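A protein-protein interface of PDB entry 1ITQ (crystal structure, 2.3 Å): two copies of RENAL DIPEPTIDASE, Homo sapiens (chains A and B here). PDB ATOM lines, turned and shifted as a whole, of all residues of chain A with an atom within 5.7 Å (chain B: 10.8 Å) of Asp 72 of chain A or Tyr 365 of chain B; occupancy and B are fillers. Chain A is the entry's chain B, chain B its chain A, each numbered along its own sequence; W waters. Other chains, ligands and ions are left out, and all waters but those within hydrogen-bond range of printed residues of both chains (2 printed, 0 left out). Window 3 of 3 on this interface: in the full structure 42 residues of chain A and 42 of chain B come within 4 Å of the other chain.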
ATOM      1  N   TRP A  25      24.959 -22.298  -4.345  1.00  0.00           N
ATOM      2  CA  TRP A  25      24.818 -23.256  -5.411  1.00  0.00           C
ATOM      3  C   TRP A  25      23.649 -24.213  -5.151  1.00  0.00           C
ATOM      4  O   TRP A  25      22.998 -24.660  -6.094  1.00  0.00           O
ATOM      5  CB  TRP A  25      26.105 -24.050  -5.599  1.00  0.00           C
ATOM      6  CG  TRP A  25      25.930 -25.118  -6.609  1.00  0.00           C
ATOM      7  CD1 TRP A  25      25.797 -26.454  -6.374  1.00  0.00           C
ATOM      8  CD2 TRP A  25      25.789 -24.940  -8.021  1.00  0.00           C
ATOM      9  NE1 TRP A  25      25.575 -27.121  -7.555  1.00  0.00           N
ATOM     10  CE2 TRP A  25      25.567 -26.214  -8.581  1.00  0.00           C
ATOM     11  CE3 TRP A  25      25.826 -23.825  -8.866  1.00  0.00           C
ATOM     12  CZ2 TRP A  25      25.385 -26.405  -9.949  1.00  0.00           C
ATOM     13  CZ3 TRP A  25      25.644 -24.015 -10.220  1.00  0.00           C
ATOM     14  CH2 TRP A  25      25.426 -25.297 -10.750  1.00  0.00           C
ATOM     15  N   LEU A  28      20.385 -22.512  -5.880  1.00  0.00           N
ATOM     16  CA  LEU A  28      20.179 -22.453  -7.324  1.00  0.00           C
ATOM     17  C   LEU A  28      19.705 -23.804  -7.812  1.00  0.00           C
ATOM     18  O   LEU A  28      18.670 -23.924  -8.461  1.00  0.00           O
ATOM     19  CB  LEU A  28      21.480 -22.102  -8.065  1.00  0.00           C
ATOM     20  CG  LEU A  28      21.442 -22.284  -9.596  1.00  0.00           C
ATOM     21  CD1 LEU A  28      20.463 -21.295 -10.221  1.00  0.00           C
ATOM     22  CD2 LEU A  28      22.822 -22.104 -10.201  1.00  0.00           C
ATOM     23  N   ASP A  29      20.484 -24.825  -7.488  1.00  0.00           N
ATOM     24  CA  ASP A  29      20.205 -26.188  -7.906  1.00  0.00           C
ATOM     25  C   ASP A  29      18.854 -26.757  -7.462  1.00  0.00           C
ATOM     26  O   ASP A  29      18.197 -27.465  -8.231  1.00  0.00           O
ATOM     27  CB  ASP A  29      21.343 -27.098  -7.437  1.00  0.00           C
ATOM     28  CG  ASP A  29      21.288 -28.469  -8.067  1.00  0.00           C
ATOM     29  OD1 ASP A  29      21.271 -29.463  -7.305  1.00  0.00           O
ATOM     30  OD2 ASP A  29      21.259 -28.544  -9.319  1.00  0.00           O
ATOM     31  N   ASN A  32      16.041 -22.875  -7.978  1.00  0.00           N
ATOM     32  CA  ASN A  32      16.284 -21.883  -9.033  1.00  0.00           C
ATOM     33  C   ASN A  32      16.310 -20.502  -8.386  1.00  0.00           C
ATOM     34  O   ASN A  32      15.767 -19.536  -8.922  1.00  0.00           O
ATOM     35  CB  ASN A  32      15.224 -21.946 -10.141  1.00  0.00           C
ATOM     36  CG  ASN A  32      15.733 -21.390 -11.473  1.00  0.00           C
ATOM     37  OD1 ASN A  32      16.828 -20.828 -11.555  1.00  0.00           O
ATOM     38  ND2 ASN A  32      14.941 -21.566 -12.527  1.00  0.00           N
ATOM     39  N   PRO A  70      29.687 -23.211 -12.588  1.00  0.00           N
ATOM     40  CA  PRO A  70      30.496 -24.278 -13.171  1.00  0.00           C
ATOM     41  C   PRO A  70      31.412 -23.861 -14.299  1.00  0.00           C
ATOM     42  O   PRO A  70      31.144 -22.902 -15.015  1.00  0.00           O
ATOM     43  CB  PRO A  70      29.440 -25.276 -13.640  1.00  0.00           C
ATOM     44  CG  PRO A  70      28.374 -25.110 -12.635  1.00  0.00           C
ATOM     45  CD  PRO A  70      28.273 -23.614 -12.554  1.00  0.00           C
ATOM     46  N   CYS A  71      32.483 -24.626 -14.465  1.00  0.00           N
ATOM     47  CA  CYS A  71      33.467 -24.385 -15.507  1.00  0.00           C
ATOM     48  C   CYS A  71      32.872 -24.391 -16.910  1.00  0.00           C
ATOM     49  O   CYS A  71      33.388 -23.724 -17.812  1.00  0.00           O
ATOM     50  CB  CYS A  71      34.584 -25.427 -15.410  1.00  0.00           C
ATOM     51  SG  CYS A  71      35.874 -24.972 -14.215  1.00  0.00           S
ATOM     52  N   ASP A  72      31.780 -25.130 -17.092  1.00  0.00           N
ATOM     53  CA  ASP A  72      31.148 -25.205 -18.403  1.00  0.00           C
ATOM     54  C   ASP A  72      30.389 -23.933 -18.792  1.00  0.00           C
ATOM     55  O   ASP A  72      29.896 -23.822 -19.912  1.00  0.00           O
ATOM     56  CB  ASP A  72      30.274 -26.463 -18.531  1.00  0.00           C
ATOM     57  CG  ASP A  72      29.049 -26.444 -17.623  1.00  0.00           C
ATOM     58  OD1 ASP A  72      28.082 -27.157 -17.940  1.00  0.00           O
ATOM     59  OD2 ASP A  72      29.037 -25.738 -16.600  1.00  0.00           O
ATOM     60  N   THR A  73      30.331 -22.967 -17.876  1.00  0.00           N
ATOM     61  CA  THR A  73      29.663 -21.699 -18.149  1.00  0.00           C
ATOM     62  C   THR A  73      30.673 -20.691 -18.690  1.00  0.00           C
ATOM     63  O   THR A  73      30.284 -19.641 -19.193  1.00  0.00           O
ATOM     64  CB  THR A  73      28.995 -21.083 -16.903  1.00  0.00           C
ATOM     65  OG1 THR A  73      30.002 -20.615 -16.005  1.00  0.00           O
ATOM     66  CG2 THR A  73      28.088 -22.095 -16.195  1.00  0.00           C
ATOM     67  N   GLN A  74      31.965 -20.991 -18.542  1.00  0.00           N
ATOM     68  CA  GLN A  74      33.026 -20.117 -19.042  1.00  0.00           C
ATOM     69  C   GLN A  74      32.842 -19.979 -20.545  1.00  0.00           C
ATOM     70  O   GLN A  74      32.659 -20.978 -21.235  1.00  0.00           O
ATOM     71  CB  GLN A  74      34.402 -20.709 -18.732  1.00  0.00           C
ATOM     72  CG  GLN A  74      35.549 -20.025 -19.472  1.00  0.00           C
ATOM     73  CD  GLN A  74      36.914 -20.335 -18.891  1.00  0.00           C
ATOM     74  OE1 GLN A  74      37.748 -19.446 -18.753  1.00  0.00           O
ATOM     75  NE2 GLN A  74      37.153 -21.598 -18.553  1.00  0.00           N
ATOM     76  N   LYS A  76      30.364 -18.633 -21.889  1.00  0.00           N
ATOM     77  CA  LYS A  76      28.930 -18.798 -22.080  1.00  0.00           C
ATOM     78  C   LYS A  76      28.202 -17.791 -21.195  1.00  0.00           C
ATOM     79  O   LYS A  76      28.250 -16.591 -21.462  1.00  0.00           O
ATOM     80  CB  LYS A  76      28.487 -20.229 -21.769  1.00  0.00           C
ATOM     81  CG  LYS A  76      28.926 -21.230 -22.812  1.00  0.00           C
ATOM     82  CD  LYS A  76      28.270 -22.567 -22.590  1.00  0.00           C
ATOM     83  CE  LYS A  76      28.757 -23.584 -23.602  1.00  0.00           C
ATOM     84  NZ  LYS A  76      28.520 -23.135 -24.999  1.00  0.00           N
ATOM     85  N   ASP A  77      27.568 -18.261 -20.125  1.00  0.00           N
ATOM     86  CA  ASP A  77      26.832 -17.367 -19.230  1.00  0.00           C
ATOM     87  C   ASP A  77      27.442 -17.210 -17.855  1.00  0.00           C
ATOM     88  O   ASP A  77      26.744 -16.890 -16.894  1.00  0.00           O
ATOM     89  CB  ASP A  77      25.356 -17.788 -19.116  1.00  0.00           C
ATOM     90  CG  ASP A  77      25.171 -19.251 -18.722  1.00  0.00           C
ATOM     91  OD1 ASP A  77      24.129 -19.555 -18.115  1.00  0.00           O
ATOM     92  OD2 ASP A  77      26.029 -20.102 -19.036  1.00  0.00           O
ATOM     93  N   ARG A  81      25.333 -15.653 -14.583  1.00  0.00           N
ATOM     94  CA  ARG A  81      25.141 -16.507 -13.410  1.00  0.00           C
ATOM     95  C   ARG A  81      25.898 -16.052 -12.164  1.00  0.00           C
ATOM     96  O   ARG A  81      25.417 -16.229 -11.043  1.00  0.00           O
ATOM     97  CB  ARG A  81      25.455 -17.961 -13.760  1.00  0.00           C
ATOM     98  CG  ARG A  81      24.493 -18.527 -14.788  1.00  0.00           C
ATOM     99  CD  ARG A  81      24.506 -20.043 -14.834  1.00  0.00           C
ATOM    100  NE  ARG A  81      23.409 -20.557 -15.651  1.00  0.00           N
ATOM    101  CZ  ARG A  81      22.155 -20.712 -15.224  1.00  0.00           C
ATOM    102  NH1 ARG A  81      21.223 -21.178 -16.048  1.00  0.00           N
ATOM    103  NH2 ARG A  81      21.830 -20.426 -13.966  1.00  0.00           N
ATOM    104  N   SER B 132      17.510 -11.399 -19.573  1.00  0.00           N
ATOM    105  CA  SER B 132      16.314 -11.974 -18.944  1.00  0.00           C
ATOM    106  C   SER B 132      16.524 -12.462 -17.519  1.00  0.00           C
ATOM    107  O   SER B 132      15.997 -13.500 -17.120  1.00  0.00           O
ATOM    108  CB  SER B 132      15.755 -13.114 -19.794  1.00  0.00           C
ATOM    109  OG  SER B 132      15.366 -12.642 -21.065  1.00  0.00           O
ATOM    110  N   SER B 133      17.275 -11.691 -16.746  1.00  0.00           N
ATOM    111  CA  SER B 133      17.547 -12.053 -15.371  1.00  0.00           C
ATOM    112  C   SER B 133      17.216 -10.923 -14.424  1.00  0.00           C
ATOM    113  O   SER B 133      17.704  -9.804 -14.569  1.00  0.00           O
ATOM    114  CB  SER B 133      19.010 -12.455 -15.207  1.00  0.00           C
ATOM    115  OG  SER B 133      19.362 -12.522 -13.836  1.00  0.00           O
ATOM    116  N   PRO B 351      11.871 -16.605 -12.280  1.00  0.00           N
ATOM    117  CA  PRO B 351      12.636 -16.548 -13.522  1.00  0.00           C
ATOM    118  C   PRO B 351      11.786 -16.705 -14.752  1.00  0.00           C
ATOM    119  O   PRO B 351      10.672 -17.212 -14.701  1.00  0.00           O
ATOM    120  CB  PRO B 351      13.600 -17.715 -13.370  1.00  0.00           C
ATOM    121  CG  PRO B 351      12.771 -18.717 -12.649  1.00  0.00           C
ATOM    122  CD  PRO B 351      12.126 -17.875 -11.575  1.00  0.00           C
ATOM    123  N   ILE B 352      12.333 -16.261 -15.868  1.00  0.00           N
ATOM    124  CA  ILE B 352      11.659 -16.349 -17.141  1.00  0.00           C
ATOM    125  C   ILE B 352      11.627 -17.835 -17.490  1.00  0.00           C
ATOM    126  O   ILE B 352      12.508 -18.588 -17.085  1.00  0.00           O
ATOM    127  CB  ILE B 352      12.456 -15.558 -18.205  1.00  0.00           C
ATOM    128  CG1 ILE B 352      11.700 -15.506 -19.533  1.00  0.00           C
ATOM    129  CG2 ILE B 352      13.857 -16.153 -18.365  1.00  0.00           C
ATOM    130  CD1 ILE B 352      12.471 -14.830 -20.634  1.00  0.00           C
ATOM    131  N   PRO B 353      10.561 -18.293 -18.159  1.00  0.00           N
ATOM    132  CA  PRO B 353      10.488 -19.710 -18.525  1.00  0.00           C
ATOM    133  C   PRO B 353      11.641 -20.101 -19.438  1.00  0.00           C
ATOM    134  O   PRO B 353      12.006 -19.355 -20.340  1.00  0.00           O
ATOM    135  CB  PRO B 353       9.144 -19.801 -19.237  1.00  0.00           C
ATOM    136  CG  PRO B 353       8.309 -18.793 -18.477  1.00  0.00           C
ATOM    137  CD  PRO B 353       9.261 -17.624 -18.360  1.00  0.00           C
ATOM    138  N   LEU B 354      12.216 -21.269 -19.177  1.00  0.00           N
ATOM    139  CA  LEU B 354      13.340 -21.797 -19.939  1.00  0.00           C
ATOM    140  C   LEU B 354      13.130 -21.783 -21.449  1.00  0.00           C
ATOM    141  O   LEU B 354      14.058 -21.509 -22.212  1.00  0.00           O
ATOM    142  CB  LEU B 354      13.641 -23.231 -19.490  1.00  0.00           C
ATOM    143  CG  LEU B 354      14.885 -23.882 -20.103  1.00  0.00           C
ATOM    144  CD1 LEU B 354      16.113 -23.114 -19.666  1.00  0.00           C
ATOM    145  CD2 LEU B 354      14.999 -25.339 -19.687  1.00  0.00           C
ATOM    146  N   LEU B 357      14.186 -18.463 -22.977  1.00  0.00           N
ATOM    147  CA  LEU B 357      15.582 -18.039 -22.975  1.00  0.00           C
ATOM    148  C   LEU B 357      16.129 -18.417 -24.340  1.00  0.00           C
ATOM    149  O   LEU B 357      15.679 -19.394 -24.941  1.00  0.00           O
ATOM    150  CB  LEU B 357      16.371 -18.763 -21.901  1.00  0.00           C
ATOM    151  CG  LEU B 357      16.214 -18.223 -20.496  1.00  0.00           C
ATOM    152  CD1 LEU B 357      17.092 -19.043 -19.574  1.00  0.00           C
ATOM    153  CD2 LEU B 357      16.624 -16.761 -20.465  1.00  0.00           C
ATOM    154  N   SER B 360      22.820 -19.952 -28.008  1.00  0.00           N
ATOM    155  CA  SER B 360      23.611 -21.146 -27.758  1.00  0.00           C
ATOM    156  C   SER B 360      24.753 -20.800 -26.810  1.00  0.00           C
ATOM    157  O   SER B 360      25.763 -21.498 -26.774  1.00  0.00           O
ATOM    158  CB  SER B 360      24.192 -21.660 -29.077  1.00  0.00           C
ATOM    159  OG  SER B 360      23.179 -21.832 -30.049  1.00  0.00           O
ATOM    160  N   CYS B 361      24.581 -19.737 -26.032  1.00  0.00           N
ATOM    161  CA  CYS B 361      25.627 -19.294 -25.121  1.00  0.00           C
ATOM    162  C   CYS B 361      25.261 -19.273 -23.662  1.00  0.00           C
ATOM    163  O   CYS B 361      25.661 -18.376 -22.928  1.00  0.00           O
ATOM    164  CB  CYS B 361      26.113 -17.919 -25.545  1.00  0.00           C
ATOM    165  SG  CYS B 361      26.928 -17.998 -27.155  1.00  0.00           S
ATOM    166  N   ARG B 362      24.526 -20.282 -23.225  1.00  0.00           N
ATOM    167  CA  ARG B 362      24.129 -20.337 -21.833  1.00  0.00           C
ATOM    168  C   ARG B 362      23.969 -21.760 -21.352  1.00  0.00           C
ATOM    169  O   ARG B 362      23.983 -22.702 -22.142  1.00  0.00           O
ATOM    170  CB  ARG B 362      22.823 -19.568 -21.625  1.00  0.00           C
ATOM    171  CG  ARG B 362      21.629 -20.132 -22.382  1.00  0.00           C
ATOM    172  CD  ARG B 362      20.357 -19.320 -22.129  1.00  0.00           C
ATOM    173  NE  ARG B 362      20.309 -18.090 -22.917  1.00  0.00           N
ATOM    174  CZ  ARG B 362      20.410 -16.869 -22.407  1.00  0.00           C
ATOM    175  NH1 ARG B 362      20.355 -15.813 -23.203  1.00  0.00           N
ATOM    176  NH2 ARG B 362      20.577 -16.701 -21.105  1.00  0.00           N
ATOM    177  N   THR B 363      23.878 -21.902 -20.036  1.00  0.00           N
ATOM    178  CA  THR B 363      23.677 -23.193 -19.395  1.00  0.00           C
ATOM    179  C   THR B 363      22.284 -23.174 -18.756  1.00  0.00           C
ATOM    180  O   THR B 363      21.678 -22.111 -18.609  1.00  0.00           O
ATOM    181  CB  THR B 363      24.769 -23.477 -18.345  1.00  0.00           C
ATOM    182  OG1 THR B 363      24.924 -22.341 -17.490  1.00  0.00           O
ATOM    183  CG2 THR B 363      26.090 -23.767 -19.029  1.00  0.00           C
ATOM    184  N   HIS B 364      21.780 -24.335 -18.356  1.00  0.00           N
ATOM    185  CA  HIS B 364      20.437 -24.386 -17.792  1.00  0.00           C
ATOM    186  C   HIS B 364      20.279 -24.817 -16.336  1.00  0.00           C
ATOM    187  O   HIS B 364      19.274 -25.434 -15.977  1.00  0.00           O
ATOM    188  CB  HIS B 364      19.543 -25.222 -18.703  1.00  0.00           C
ATOM    189  CG  HIS B 364      19.468 -24.699 -20.105  1.00  0.00           C
ATOM    190  ND1 HIS B 364      19.529 -25.519 -21.212  1.00  0.00           N
ATOM    191  CD2 HIS B 364      19.358 -23.435 -20.579  1.00  0.00           C
ATOM    192  CE1 HIS B 364      19.459 -24.783 -22.307  1.00  0.00           C
ATOM    193  NE2 HIS B 364      19.355 -23.515 -21.951  1.00  0.00           N
ATOM    194  N   TYR B 365      21.235 -24.436 -15.492  1.00  0.00           N
ATOM    195  CA  TYR B 365      21.186 -24.773 -14.072  1.00  0.00           C
ATOM    196  C   TYR B 365      20.056 -24.027 -13.380  1.00  0.00           C
ATOM    197  O   TYR B 365      19.830 -22.844 -13.643  1.00  0.00           O
ATOM    198  CB  TYR B 365      22.506 -24.427 -13.390  1.00  0.00           C
ATOM    199  CG  TYR B 365      23.688 -25.164 -13.950  1.00  0.00           C
ATOM    200  CD1 TYR B 365      23.843 -26.534 -13.737  1.00  0.00           C
ATOM    201  CD2 TYR B 365      24.666 -24.493 -14.686  1.00  0.00           C
ATOM    202  CE1 TYR B 365      24.947 -27.223 -14.246  1.00  0.00           C
ATOM    203  CE2 TYR B 365      25.770 -25.167 -15.199  1.00  0.00           C
ATOM    204  CZ  TYR B 365      25.905 -26.530 -14.975  1.00  0.00           C
ATOM    205  OH  TYR B 365      26.995 -27.198 -15.474  1.00  0.00           O
ATOM    206  N   GLY B 366      19.373 -24.715 -12.471  1.00  0.00           N
ATOM    207  CA  GLY B 366      18.264 -24.120 -11.754  1.00  0.00           C
ATOM    208  C   GLY B 366      16.926 -24.545 -12.329  1.00  0.00           C
ATOM    209  O   GLY B 366      15.951 -24.707 -11.596  1.00  0.00           O
ATOM    210  N   TYR B 367      16.874 -24.693 -13.648  1.00  0.00           N
ATOM    211  CA  TYR B 367      15.656 -25.111 -14.327  1.00  0.00           C
ATOM    212  C   TYR B 367      15.517 -26.617 -14.258  1.00  0.00           C
ATOM    213  O   TYR B 367      16.468 -27.348 -14.543  1.00  0.00           O
ATOM    214  CB  TYR B 367      15.675 -24.663 -15.785  1.00  0.00           C
ATOM    215  CG  TYR B 367      15.537 -23.179 -15.938  1.00  0.00           C
ATOM    216  CD1 TYR B 367      14.356 -22.538 -15.576  1.00  0.00           C
ATOM    217  CD2 TYR B 367      16.588 -22.409 -16.416  1.00  0.00           C
ATOM    218  CE1 TYR B 367      14.227 -21.167 -15.685  1.00  0.00           C
ATOM    219  CE2 TYR B 367      16.472 -21.033 -16.531  1.00  0.00           C
ATOM    220  CZ  TYR B 367      15.287 -20.419 -16.161  1.00  0.00           C
ATOM    221  OH  TYR B 367      15.164 -19.058 -16.262  1.00  0.00           O
ATOM    222  N   SER B 368      14.325 -27.079 -13.902  1.00  0.00           N
ATOM    223  CA  SER B 368      14.069 -28.507 -13.784  1.00  0.00           C
ATOM    224  C   SER B 368      12.573 -28.810 -13.754  1.00  0.00           C
ATOM    225  O   SER B 368      11.977 -29.168 -14.775  1.00  0.00           O
ATOM    226  CB  SER B 368      14.745 -29.049 -12.517  1.00  0.00           C
ATOM    227  OG  SER B 368      14.425 -28.252 -11.384  1.00  0.00           O
ATOM    228  N   SER B 369      11.982 -28.673 -12.569  1.00  0.00           N
ATOM    229  CA  SER B 369      10.560 -28.922 -12.365  1.00  0.00           C
ATOM    230  C   SER B 369       9.854 -27.656 -11.866  1.00  0.00           C
ATOM    231  O   SER B 369      10.380 -27.005 -10.931  1.00  0.00           O
ATOM    232  CB  SER B 369      10.356 -30.088 -11.381  1.00  0.00           C
ATOM    233  OG  SER B 369      11.005 -29.859 -10.137  1.00  0.00           O
ATOM    234  OXT SER B 369       8.794 -27.316 -12.439  1.00  0.00           O
HETATM  235  O   HOH W   1      21.246 -18.395 -18.587  1.00  0.00           O
HETATM  236  O   HOH W   2      25.334 -15.564 -23.047  1.00  0.00           O
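Water W2 bridges O of Cys 361 of chain B and O of Lys 76 of chain A. Water W1 lies within hydrogen-bond range of the guanidinium group (NH2) of Arg 362 of chain B (3.1 Å) and the side-chain carboxylate (OD1) of Asp 77 of chain A (3.1 Å).
Hydrophobic or aromatic side chains of chain A that line the printed part of chain B: Trp 25, Leu 28 and Pro 70. Of the 17 printed residues of chain B, 9 touch a printed residue of chain A. Among the printed residues, no Asp or Glu carboxylate lies within 4 Å of a Lys or Arg side-chain nitrogen of the other chain.
The backbone carbonyl oxygen of Tyr 365 of chain B sits at hydrogen-bond distance from the guanidinium group of Arg 81 of chain A (3.2 Å). The side-chain amide nitrogen (ND2) of Asn 32 of chain A sits close to the backbone carbonyl oxygen (O) of Gly 366 of chain B (3.4 Å). The backbone NH (N) of Asp 77 of chain A lies within hydrogen-bond range of the backbone carbonyl oxygen (O) of Cys 361 of chain B (3.4 Å). The guanidinium group (NH1) of Arg 81 of chain A sits at hydrogen-bond distance from the backbone carbonyl oxygen (O) of Thr 363 of chain B. The side-chain hydroxyl of Tyr 365 of chain B is in hydrogen-bond range of the side-chain carboxylate of Asp 72 of chain A, at 2.7 Å. The backbone carbonyl oxygen (O) of Cys 361 of chain B lies close to the backbone carbonyl oxygen (O) of Lys 76 of chain A, at 3.5 Å. The side-chain hydroxyl (OG1) of Thr 363 of chain B sits at hydrogen-bond distance from the side-chain carboxylate (OD2) of Asp 77 of chain A (2.9 Å).
The guanidinium group (NE) of Arg 81 of chain A is in salt-bridge range of the side-chain carboxylate (OD1) of Asp 77 of chain A (2.8 Å). The side-chain hydroxyl (OG1) of Thr 73 of chain A lies within hydrogen-bond range of the backbone carbonyl oxygen (O) of Pro 70 of chain A, 2.7 Å away. The side-chain hydroxyl of Tyr 367 of chain B lies within hydrogen-bond range of the backbone carbonyl oxygen of Ile 352 of chain B.
Cys 71 of chain A touches none of the printed residues of chain B. Of chain B, only Thr 363 and Tyr 365 come within 4 Å of Asp 72 of chain A. Printed residues of chain B within 4 Å of Lys 76 of chain A: Ser 360 and Cys 361. Of the printed residues of chain A, Ser 360 of chain B touches Lys 76 (3.7 Å). Of the printed residues of chain A, Tyr 367 of chain B touches Asn 32.
No position is printed for both chains.
Among the printed residues, pairs that only touch across the chains: Trp 25 of chain A with Tyr 365 of chain B (3.6 Å), Leu 28 of chain A with Tyr 365 of chain B (3.8 Å), Leu 28 of chain A with Gly 366 of chain B (3.3 Å), Asn 32 of chain A with Pro 351 of chain B (3.6 Å), Asn 32 of chain A with Tyr 367 of chain B (3.3 Å), Pro 70 of chain A with Tyr 365 of chain B (3.6 Å), Asp 72 of chain A with Thr 363 of chain B (3.9 Å), Thr 73 of chain A with Thr 363 of chain B (3.4 Å), Thr 73 of chain A with Tyr 365 of chain B (3.98 Å), Lys 76 of chain A with Ser 360 of chain B (3.7 Å), Asp 77 of chain A with Arg 362 of chain B (3.4 Å) and Arg 81 of chain A with His 364 of chain B (3.7 Å).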
